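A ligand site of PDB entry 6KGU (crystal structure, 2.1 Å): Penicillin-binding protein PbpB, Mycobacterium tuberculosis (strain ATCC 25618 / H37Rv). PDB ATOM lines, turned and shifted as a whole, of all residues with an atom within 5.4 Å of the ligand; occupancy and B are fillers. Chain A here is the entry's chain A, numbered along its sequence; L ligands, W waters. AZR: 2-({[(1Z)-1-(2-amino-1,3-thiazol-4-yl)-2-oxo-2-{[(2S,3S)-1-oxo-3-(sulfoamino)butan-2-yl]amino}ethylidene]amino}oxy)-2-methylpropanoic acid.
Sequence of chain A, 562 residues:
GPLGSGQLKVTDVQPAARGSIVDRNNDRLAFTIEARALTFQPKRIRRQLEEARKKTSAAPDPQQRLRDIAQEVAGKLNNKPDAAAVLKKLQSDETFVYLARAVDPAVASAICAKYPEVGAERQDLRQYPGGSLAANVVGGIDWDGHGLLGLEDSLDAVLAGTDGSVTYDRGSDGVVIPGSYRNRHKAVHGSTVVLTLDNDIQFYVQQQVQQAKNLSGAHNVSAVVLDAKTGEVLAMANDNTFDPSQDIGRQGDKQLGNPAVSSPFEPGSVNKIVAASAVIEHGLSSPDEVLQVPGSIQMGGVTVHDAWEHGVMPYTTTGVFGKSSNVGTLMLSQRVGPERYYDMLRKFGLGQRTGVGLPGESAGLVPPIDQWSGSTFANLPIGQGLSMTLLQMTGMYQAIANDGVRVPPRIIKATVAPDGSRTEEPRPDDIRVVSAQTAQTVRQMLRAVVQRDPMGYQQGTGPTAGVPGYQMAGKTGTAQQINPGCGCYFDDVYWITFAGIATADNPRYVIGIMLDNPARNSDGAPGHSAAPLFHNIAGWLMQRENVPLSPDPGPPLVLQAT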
ATOM      1  N   GLU A 266      23.800  23.169  -0.724  1.00  0.00           N
ATOM      2  CA  GLU A 266      23.529  21.886  -1.395  1.00  0.00           C
ATOM      3  C   GLU A 266      23.220  20.842  -0.327  1.00  0.00           C
ATOM      4  O   GLU A 266      24.055  20.636   0.560  1.00  0.00           O
ATOM      5  CB  GLU A 266      24.713  21.408  -2.250  1.00  0.00           C
ATOM      6  CG  GLU A 266      24.694  21.863  -3.684  1.00  0.00           C
ATOM      7  CD  GLU A 266      25.419  20.905  -4.627  1.00  0.00           C
ATOM      8  OE1 GLU A 266      26.378  20.209  -4.211  1.00  0.00           O
ATOM      9  OE2 GLU A 266      25.025  20.832  -5.800  1.00  0.00           O
ATOM     10  N   PRO A 267      22.071  20.179  -0.364  1.00  0.00           N
ATOM     11  CA  PRO A 267      21.705  19.300   0.759  1.00  0.00           C
ATOM     12  C   PRO A 267      22.436  17.967   0.799  1.00  0.00           C
ATOM     13  O   PRO A 267      22.568  17.361   1.866  1.00  0.00           O
ATOM     14  CB  PRO A 267      20.202  19.074   0.521  1.00  0.00           C
ATOM     15  CG  PRO A 267      20.070  19.148  -0.986  1.00  0.00           C
ATOM     16  CD  PRO A 267      21.002  20.270  -1.377  1.00  0.00           C
ATOM     17  N   GLY A 268      22.866  17.446  -0.344  1.00  0.00           N
ATOM     18  CA  GLY A 268      23.320  16.054  -0.329  1.00  0.00           C
ATOM     19  C   GLY A 268      22.200  15.142   0.150  1.00  0.00           C
ATOM     20  O   GLY A 268      21.029  15.368  -0.142  1.00  0.00           O
ATOM     21  N   SER A 269      22.565  14.138   0.962  1.00  0.00           N
ATOM     22  CA  SER A 269      21.696  12.979   1.178  1.00  0.00           C
ATOM     23  C   SER A 269      20.426  13.271   1.981  1.00  0.00           C
ATOM     24  O   SER A 269      19.512  12.414   1.990  1.00  0.00           O
ATOM     25  CB  SER A 269      22.464  11.857   1.878  1.00  0.00           C
ATOM     26  OG  SER A 269      23.400  11.277   0.971  1.00  0.00           O
ATOM     27  N   VAL A 270      20.319  14.406   2.681  1.00  0.00           N
ATOM     28  CA  VAL A 270      19.051  14.664   3.351  1.00  0.00           C
ATOM     29  C   VAL A 270      17.957  14.838   2.314  1.00  0.00           C
ATOM     30  O   VAL A 270      16.775  14.625   2.621  1.00  0.00           O
ATOM     31  CB  VAL A 270      19.076  15.890   4.285  1.00  0.00           C
ATOM     32  CG1 VAL A 270      19.822  15.554   5.559  1.00  0.00           C
ATOM     33  CG2 VAL A 270      19.631  17.152   3.577  1.00  0.00           C
ATOM     34  N   LYS A 272      17.282  12.811   0.108  1.00  0.00           N
ATOM     35  CA  LYS A 272      16.788  11.514  -0.322  1.00  0.00           C
ATOM     36  C   LYS A 272      15.362  11.248   0.167  1.00  0.00           C
ATOM     37  O   LYS A 272      14.691  10.360  -0.374  1.00  0.00           O
ATOM     38  CB  LYS A 272      17.731  10.400   0.145  1.00  0.00           C
ATOM     39  CG  LYS A 272      19.076  10.416  -0.611  1.00  0.00           C
ATOM     40  CD  LYS A 272      19.990   9.257  -0.211  1.00  0.00           C
ATOM     41  CE  LYS A 272      21.377   9.362  -0.840  1.00  0.00           C
ATOM     42  NZ  LYS A 272      22.268   8.230  -0.405  1.00  0.00           N
ATOM     43  N   ALA A 307      29.570   5.878  -1.249  1.00  0.00           N
ATOM     44  CA  ALA A 307      30.651   6.417  -0.423  1.00  0.00           C
ATOM     45  C   ALA A 307      31.526   5.320   0.199  1.00  0.00           C
ATOM     46  O   ALA A 307      32.446   5.648   0.965  1.00  0.00           O
ATOM     47  CB  ALA A 307      30.091   7.302   0.683  1.00  0.00           C
ATOM     48  N   LYS A 323      21.480   3.141   4.839  1.00  0.00           N
ATOM     49  CA  LYS A 323      22.925   3.181   4.605  1.00  0.00           C
ATOM     50  C   LYS A 323      23.346   4.322   3.693  1.00  0.00           C
ATOM     51  O   LYS A 323      24.542   4.598   3.579  1.00  0.00           O
ATOM     52  CB  LYS A 323      23.421   1.849   4.016  1.00  0.00           C
ATOM     53  CG  LYS A 323      23.345   0.686   5.010  1.00  0.00           C
ATOM     54  CD  LYS A 323      24.193  -0.514   4.618  1.00  0.00           C
ATOM     55  CE  LYS A 323      23.961  -1.705   5.557  1.00  0.00           C
ATOM     56  NZ  LYS A 323      24.398  -1.420   6.972  1.00  0.00           N
ATOM     57  N   SER A 324      22.375   4.974   3.045  1.00  0.00           N
ATOM     58  CA  SER A 324      22.606   6.110   2.145  1.00  0.00           C
ATOM     59  C   SER A 324      23.415   5.675   0.920  1.00  0.00           C
ATOM     60  O   SER A 324      24.484   6.211   0.621  1.00  0.00           O
ATOM     61  CB  SER A 324      23.265   7.274   2.878  1.00  0.00           C
ATOM     62  OG  SER A 324      22.923   8.524   2.272  1.00  0.00           O
ATOM     63  N   ASN A 326      23.884   6.058  -2.721  1.00  0.00           N
ATOM     64  CA  ASN A 326      23.558   6.912  -3.859  1.00  0.00           C
ATOM     65  C   ASN A 326      23.101   6.073  -5.054  1.00  0.00           C
ATOM     66  O   ASN A 326      22.148   6.432  -5.744  1.00  0.00           O
ATOM     67  CB  ASN A 326      24.760   7.767  -4.283  1.00  0.00           C
ATOM     68  CG  ASN A 326      25.131   8.854  -3.269  1.00  0.00           C
ATOM     69  OD1 ASN A 326      24.375   9.155  -2.341  1.00  0.00           O
ATOM     70  ND2 ASN A 326      26.289   9.449  -3.470  1.00  0.00           N
ATOM     71  N   ILE A 382      20.135  12.565  -5.256  1.00  0.00           N
ATOM     72  CA  ILE A 382      21.052  12.421  -4.127  1.00  0.00           C
ATOM     73  C   ILE A 382      21.437  13.782  -3.534  1.00  0.00           C
ATOM     74  O   ILE A 382      22.369  13.862  -2.727  1.00  0.00           O
ATOM     75  CB  ILE A 382      22.289  11.596  -4.524  1.00  0.00           C
ATOM     76  CG1 ILE A 382      22.992  12.165  -5.753  1.00  0.00           C
ATOM     77  CG2 ILE A 382      21.863  10.162  -4.847  1.00  0.00           C
ATOM     78  CD1 ILE A 382      24.007  13.238  -5.479  1.00  0.00           C
ATOM     79  N   GLY A 383      20.724  14.850  -3.890  1.00  0.00           N
ATOM     80  CA  GLY A 383      20.941  16.138  -3.271  1.00  0.00           C
ATOM     81  C   GLY A 383      22.044  16.981  -3.871  1.00  0.00           C
ATOM     82  O   GLY A 383      22.559  17.878  -3.182  1.00  0.00           O
ATOM     83  N   GLN A 384      22.426  16.749  -5.120  1.00  0.00           N
ATOM     84  CA  GLN A 384      23.442  17.545  -5.787  1.00  0.00           C
ATOM     85  C   GLN A 384      22.781  18.330  -6.910  1.00  0.00           C
ATOM     86  O   GLN A 384      21.911  17.804  -7.599  1.00  0.00           O
ATOM     87  CB  GLN A 384      24.563  16.660  -6.359  1.00  0.00           C
ATOM     88  CG  GLN A 384      25.758  17.428  -6.925  1.00  0.00           C
ATOM     89  CD  GLN A 384      26.737  16.520  -7.676  1.00  0.00           C
ATOM     90  OE1 GLN A 384      27.097  15.436  -7.200  1.00  0.00           O
ATOM     91  NE2 GLN A 384      27.186  16.963  -8.846  1.00  0.00           N
ATOM     92  N   THR A 461      23.443   4.969   9.013  1.00  0.00           N
ATOM     93  CA  THR A 461      24.512   5.957   9.022  1.00  0.00           C
ATOM     94  C   THR A 461      24.549   6.804  10.288  1.00  0.00           C
ATOM     95  O   THR A 461      25.579   7.427  10.567  1.00  0.00           O
ATOM     96  CB  THR A 461      24.390   6.883   7.800  1.00  0.00           C
ATOM     97  OG1 THR A 461      23.069   7.474   7.809  1.00  0.00           O
ATOM     98  CG2 THR A 461      24.623   6.129   6.481  1.00  0.00           C
ATOM     99  N   LYS A 475      17.567  11.349   8.836  1.00  0.00           N
ATOM    100  CA  LYS A 475      18.448  11.145   7.696  1.00  0.00           C
ATOM    101  C   LYS A 475      19.667  12.044   7.849  1.00  0.00           C
ATOM    102  O   LYS A 475      19.532  13.237   8.160  1.00  0.00           O
ATOM    103  CB  LYS A 475      17.739  11.443   6.364  1.00  0.00           C
ATOM    104  CG  LYS A 475      18.590  11.181   5.126  1.00  0.00           C
ATOM    105  CD  LYS A 475      18.814   9.687   4.933  1.00  0.00           C
ATOM    106  CE  LYS A 475      19.822   9.401   3.850  1.00  0.00           C
ATOM    107  NZ  LYS A 475      21.233   9.558   4.315  1.00  0.00           N
ATOM    108  N   THR A 476      20.849  11.471   7.611  1.00  0.00           N
ATOM    109  CA  THR A 476      22.138  12.156   7.625  1.00  0.00           C
ATOM    110  C   THR A 476      22.429  12.735   6.252  1.00  0.00           C
ATOM    111  O   THR A 476      21.957  12.231   5.222  1.00  0.00           O
ATOM    112  CB  THR A 476      23.250  11.180   7.986  1.00  0.00           C
ATOM    113  OG1 THR A 476      23.040   9.951   7.276  1.00  0.00           O
ATOM    114  CG2 THR A 476      23.302  10.909   9.512  1.00  0.00           C
ATOM    115  N   GLY A 477      23.242  13.801   6.226  1.00  0.00           N
ATOM    116  CA  GLY A 477      23.771  14.320   4.984  1.00  0.00           C
ATOM    117  C   GLY A 477      25.227  14.740   5.103  1.00  0.00           C
ATOM    118  O   GLY A 477      25.642  15.312   6.114  1.00  0.00           O
ATOM    119  N   THR A 478      26.004  14.475   4.050  1.00  0.00           N
ATOM    120  CA  THR A 478      27.420  14.856   3.952  1.00  0.00           C
ATOM    121  C   THR A 478      27.625  15.295   2.499  1.00  0.00           C
ATOM    122  O   THR A 478      27.803  14.453   1.612  1.00  0.00           O
ATOM    123  CB  THR A 478      28.355  13.705   4.307  1.00  0.00           C
ATOM    124  OG1 THR A 478      27.984  13.142   5.582  1.00  0.00           O
ATOM    125  CG2 THR A 478      29.828  14.169   4.374  1.00  0.00           C
ATOM    126  N   ALA A 479      27.601  16.606   2.266  1.00  0.00           N
ATOM    127  CA  ALA A 479      27.664  17.170   0.922  1.00  0.00           C
ATOM    128  C   ALA A 479      29.005  17.867   0.734  1.00  0.00           C
ATOM    129  O   ALA A 479      29.368  18.756   1.520  1.00  0.00           O
ATOM    130  CB  ALA A 479      26.518  18.151   0.678  1.00  0.00           C
ATOM    131  N   GLN A 480      29.741  17.444  -0.286  1.00  0.00           N
ATOM    132  CA  GLN A 480      30.959  18.127  -0.707  1.00  0.00           C
ATOM    133  C   GLN A 480      30.658  19.581  -1.051  1.00  0.00           C
ATOM    134  O   GLN A 480      29.696  19.874  -1.762  1.00  0.00           O
ATOM    135  CB  GLN A 480      31.547  17.394  -1.904  1.00  0.00           C
ATOM    136  CG  GLN A 480      32.987  17.636  -2.122  1.00  0.00           C
ATOM    137  CD  GLN A 480      33.818  17.090  -0.980  1.00  0.00           C
ATOM    138  OE1 GLN A 480      33.715  15.908  -0.641  1.00  0.00           O
ATOM    139  NE2 GLN A 480      34.647  17.947  -0.376  1.00  0.00           N
ATOM    140  N   GLN A 481      31.475  20.508  -0.544  1.00  0.00           N
ATOM    141  CA  GLN A 481      31.267  21.923  -0.833  1.00  0.00           C
ATOM    142  C   GLN A 481      32.039  22.357  -2.079  1.00  0.00           C
ATOM    143  O   GLN A 481      33.064  21.775  -2.432  1.00  0.00           O
ATOM    144  CB  GLN A 481      31.688  22.806   0.348  1.00  0.00           C
ATOM    145  CG  GLN A 481      30.621  22.907   1.456  1.00  0.00           C
ATOM    146  CD  GLN A 481      31.008  23.874   2.565  1.00  0.00           C
ATOM    147  OE1 GLN A 481      30.919  23.570   3.758  1.00  0.00           O
ATOM    148  NE2 GLN A 481      31.423  25.056   2.183  1.00  0.00           N
ATOM    149  N   TYR A 489      34.425  21.249  -6.911  1.00  0.00           N
ATOM    150  CA  TYR A 489      34.212  20.727  -5.560  1.00  0.00           C
ATOM    151  C   TYR A 489      35.519  20.641  -4.801  1.00  0.00           C
ATOM    152  O   TYR A 489      36.563  20.290  -5.354  1.00  0.00           O
ATOM    153  CB  TYR A 489      33.546  19.360  -5.608  1.00  0.00           C
ATOM    154  CG  TYR A 489      32.062  19.437  -5.830  1.00  0.00           C
ATOM    155  CD1 TYR A 489      31.218  19.923  -4.830  1.00  0.00           C
ATOM    156  CD2 TYR A 489      31.490  19.060  -7.042  1.00  0.00           C
ATOM    157  CE1 TYR A 489      29.854  20.014  -5.022  1.00  0.00           C
ATOM    158  CE2 TYR A 489      30.123  19.151  -7.253  1.00  0.00           C
ATOM    159  CZ  TYR A 489      29.304  19.635  -6.238  1.00  0.00           C
ATOM    160  OH  TYR A 489      27.938  19.726  -6.439  1.00  0.00           O
ATOM    161  N   ASP A 491      37.761  18.679  -1.930  1.00  0.00           N
ATOM    162  CA  ASP A 491      37.972  17.274  -1.661  1.00  0.00           C
ATOM    163  C   ASP A 491      37.529  16.889  -0.268  1.00  0.00           C
ATOM    164  O   ASP A 491      37.068  15.758  -0.049  1.00  0.00           O
ATOM    165  CB  ASP A 491      39.465  16.951  -1.864  1.00  0.00           C
ATOM    166  CG  ASP A 491      39.810  15.503  -1.558  1.00  0.00           C
ATOM    167  OD1 ASP A 491      39.404  14.618  -2.337  1.00  0.00           O
ATOM    168  OD2 ASP A 491      40.512  15.256  -0.548  1.00  0.00           O
ATOM    169  N   TYR A 494      32.860  19.901   3.810  1.00  0.00           N
ATOM    170  CA  TYR A 494      31.491  19.388   3.764  1.00  0.00           C
ATOM    171  C   TYR A 494      30.478  20.309   4.420  1.00  0.00           C
ATOM    172  O   TYR A 494      30.785  21.034   5.373  1.00  0.00           O
ATOM    173  CB  TYR A 494      31.369  18.045   4.457  1.00  0.00           C
ATOM    174  CG  TYR A 494      32.433  17.067   4.065  1.00  0.00           C
ATOM    175  CD1 TYR A 494      33.180  16.417   5.025  1.00  0.00           C
ATOM    176  CD2 TYR A 494      32.684  16.800   2.726  1.00  0.00           C
ATOM    177  CE1 TYR A 494      34.169  15.520   4.669  1.00  0.00           C
ATOM    178  CE2 TYR A 494      33.663  15.909   2.361  1.00  0.00           C
ATOM    179  CZ  TYR A 494      34.400  15.278   3.334  1.00  0.00           C
ATOM    180  OH  TYR A 494      35.369  14.391   2.961  1.00  0.00           O
HETATM  181  C7  AZR L   1      27.533   9.350   1.653  1.00  0.00           C
HETATM  182  S8  AZR L   1      25.969  16.181  -3.121  1.00  0.00           S
HETATM  183  O9  AZR L   1      24.820  12.930   1.802  1.00  0.00           O
HETATM  184  O10 AZR L   1      27.175  11.269  -1.934  1.00  0.00           O
HETATM  185  O11 AZR L   1      29.845  12.147  -0.527  1.00  0.00           O
HETATM  186  N12 AZR L   1      25.421   9.986   2.782  1.00  0.00           N
HETATM  187  N13 AZR L   1      26.910  12.143   0.155  1.00  0.00           N
HETATM  188  N14 AZR L   1      29.455  13.366  -1.156  1.00  0.00           N
HETATM  189  N15 AZR L   1      28.335  15.730  -2.166  1.00  0.00           N
HETATM  190  N16 AZR L   1      27.992  17.947  -2.907  1.00  0.00           N
HETATM  191  S17 AZR L   1      25.483  10.064   4.377  1.00  0.00           S
HETATM  192  C18 AZR L   1      26.537  10.455   1.936  1.00  0.00           C
HETATM  193  C19 AZR L   1      25.990  11.140   0.669  1.00  0.00           C
HETATM  194  C20 AZR L   1      24.739  11.920   1.137  1.00  0.00           C
HETATM  195  C21 AZR L   1      27.366  12.156  -1.109  1.00  0.00           C
HETATM  196  C22 AZR L   1      28.210  13.346  -1.432  1.00  0.00           C
HETATM  197  C23 AZR L   1      31.207  12.130  -0.140  1.00  0.00           C
HETATM  198  C24 AZR L   1      27.602  14.554  -2.055  1.00  0.00           C
HETATM  199  C25 AZR L   1      26.330  14.606  -2.517  1.00  0.00           C
HETATM  200  C26 AZR L   1      27.587  16.678  -2.702  1.00  0.00           C
HETATM  201  C27 AZR L   1      31.331  13.116   1.014  1.00  0.00           C
HETATM  202  C28 AZR L   1      31.618  10.734   0.288  1.00  0.00           C
HETATM  203  C29 AZR L   1      32.035  12.581  -1.334  1.00  0.00           C
HETATM  204  O30 AZR L   1      31.637  12.571  -2.474  1.00  0.00           O
HETATM  205  O31 AZR L   1      33.245  12.939  -1.002  1.00  0.00           O
HETATM  206  O32 AZR L   1      26.410   9.086   4.831  1.00  0.00           O
HETATM  207  O33 AZR L   1      24.102   9.575   4.882  1.00  0.00           O
HETATM  208  O34 AZR L   1      25.602  11.426   4.741  1.00  0.00           O
HETATM  209  O   HOH W   1      24.269  12.007  -1.835  1.00  0.00           O
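ND2 of Asn 326 sits at hydrogen-bond distance from O10 of the ligand.
The side-chain hydroxyl (OG1) of Thr 476 is in hydrogen-bond range of an oxygen (O33) of the ligand, 2.6 Å away.
An oxygen (O9) of the ligand lies close to the backbone NH (N) of Ser 269 (2.7 Å).
A nitrogen (N13) of the ligand lies within hydrogen-bond range of the backbone carbonyl oxygen (O) of Thr 478, 2.9 Å away.
An oxygen (O9) of the ligand lies within hydrogen-bond range of the backbone NH (N) of Thr 478 (3.0 Å).
The side-chain hydroxyl (OG) of Ser 269 is covalently linked to a carbon (C20) of the ligand.
A nitrogen (N16) of the ligand lies within hydrogen-bond range of the backbone carbonyl oxygen (O) of Gln 480, 2.8 Å away.
NZ of Lys 475 is in salt-bridge range of O33 of the ligand (2.9 Å).
The side-chain hydroxyl (OG) of Ser 324 lies within hydrogen-bond range of a nitrogen (N12) of the ligand (2.9 Å).
OE1 of Glu 266 lies within hydrogen-bond range of N16 of the ligand, 3.1 Å away.
The side-chain amide oxygen (OE1) of Gln 480 sits close to an oxygen (O31) of the ligand, 3.0 Å away.
N of Gln 480 lies within hydrogen-bond range of N15 of the ligand.
OG1 of Thr 478 sits at hydrogen-bond distance from O34 of the ligand.
Residues that only touch the ligand: Gly 477 (3.4 Å), Ala 307 (3.4 Å), Ala 479 (3.5 Å), Tyr 489 (3.5 Å), Gln 384 (3.6 Å), Thr 461 (3.7 Å), Gly 268 (3.8 Å), Gly 383 (3.8 Å) and Tyr 494 (3.9 Å).
17 residues have an atom within 4 Å of the ligand: Glu 266, Gly 268, Ser 269, Ala 307, Ser 324, Asn 326, Gly 383, Gln 384, Thr 461, Lys 475, Thr 476, Gly 477, Thr 478, Ala 479, Gln 480, Tyr 489 and Tyr 494.
The side-chain amide oxygen (OD1) of Asn 326 is in hydrogen-bond range of the side-chain amino group (NZ) of Lys 272, at 3.0 Å.
O of Tyr 494 lies close to OE1 of Gln 481 (3.0 Å).
OG of Ser 324 sits at hydrogen-bond distance from NZ of Lys 272 (2.8 Å).
The side-chain amino group (NZ) of Lys 475 is in hydrogen-bond range of the side-chain hydroxyl (OG) of Ser 324 (2.8 Å).
The side-chain amino group of Lys 475 is in hydrogen-bond range of the side-chain hydroxyl of Thr 476 (3.5 Å).
The side-chain hydroxyl of Ser 269 lies within hydrogen-bond range of the side-chain hydroxyl of Ser 324 (3.1 Å).
OG1 of Thr 476 is in hydrogen-bond range of OG1 of Thr 461, 2.5 Å away.
N of Gly 268 is in hydrogen-bond range of O of Gly 383.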
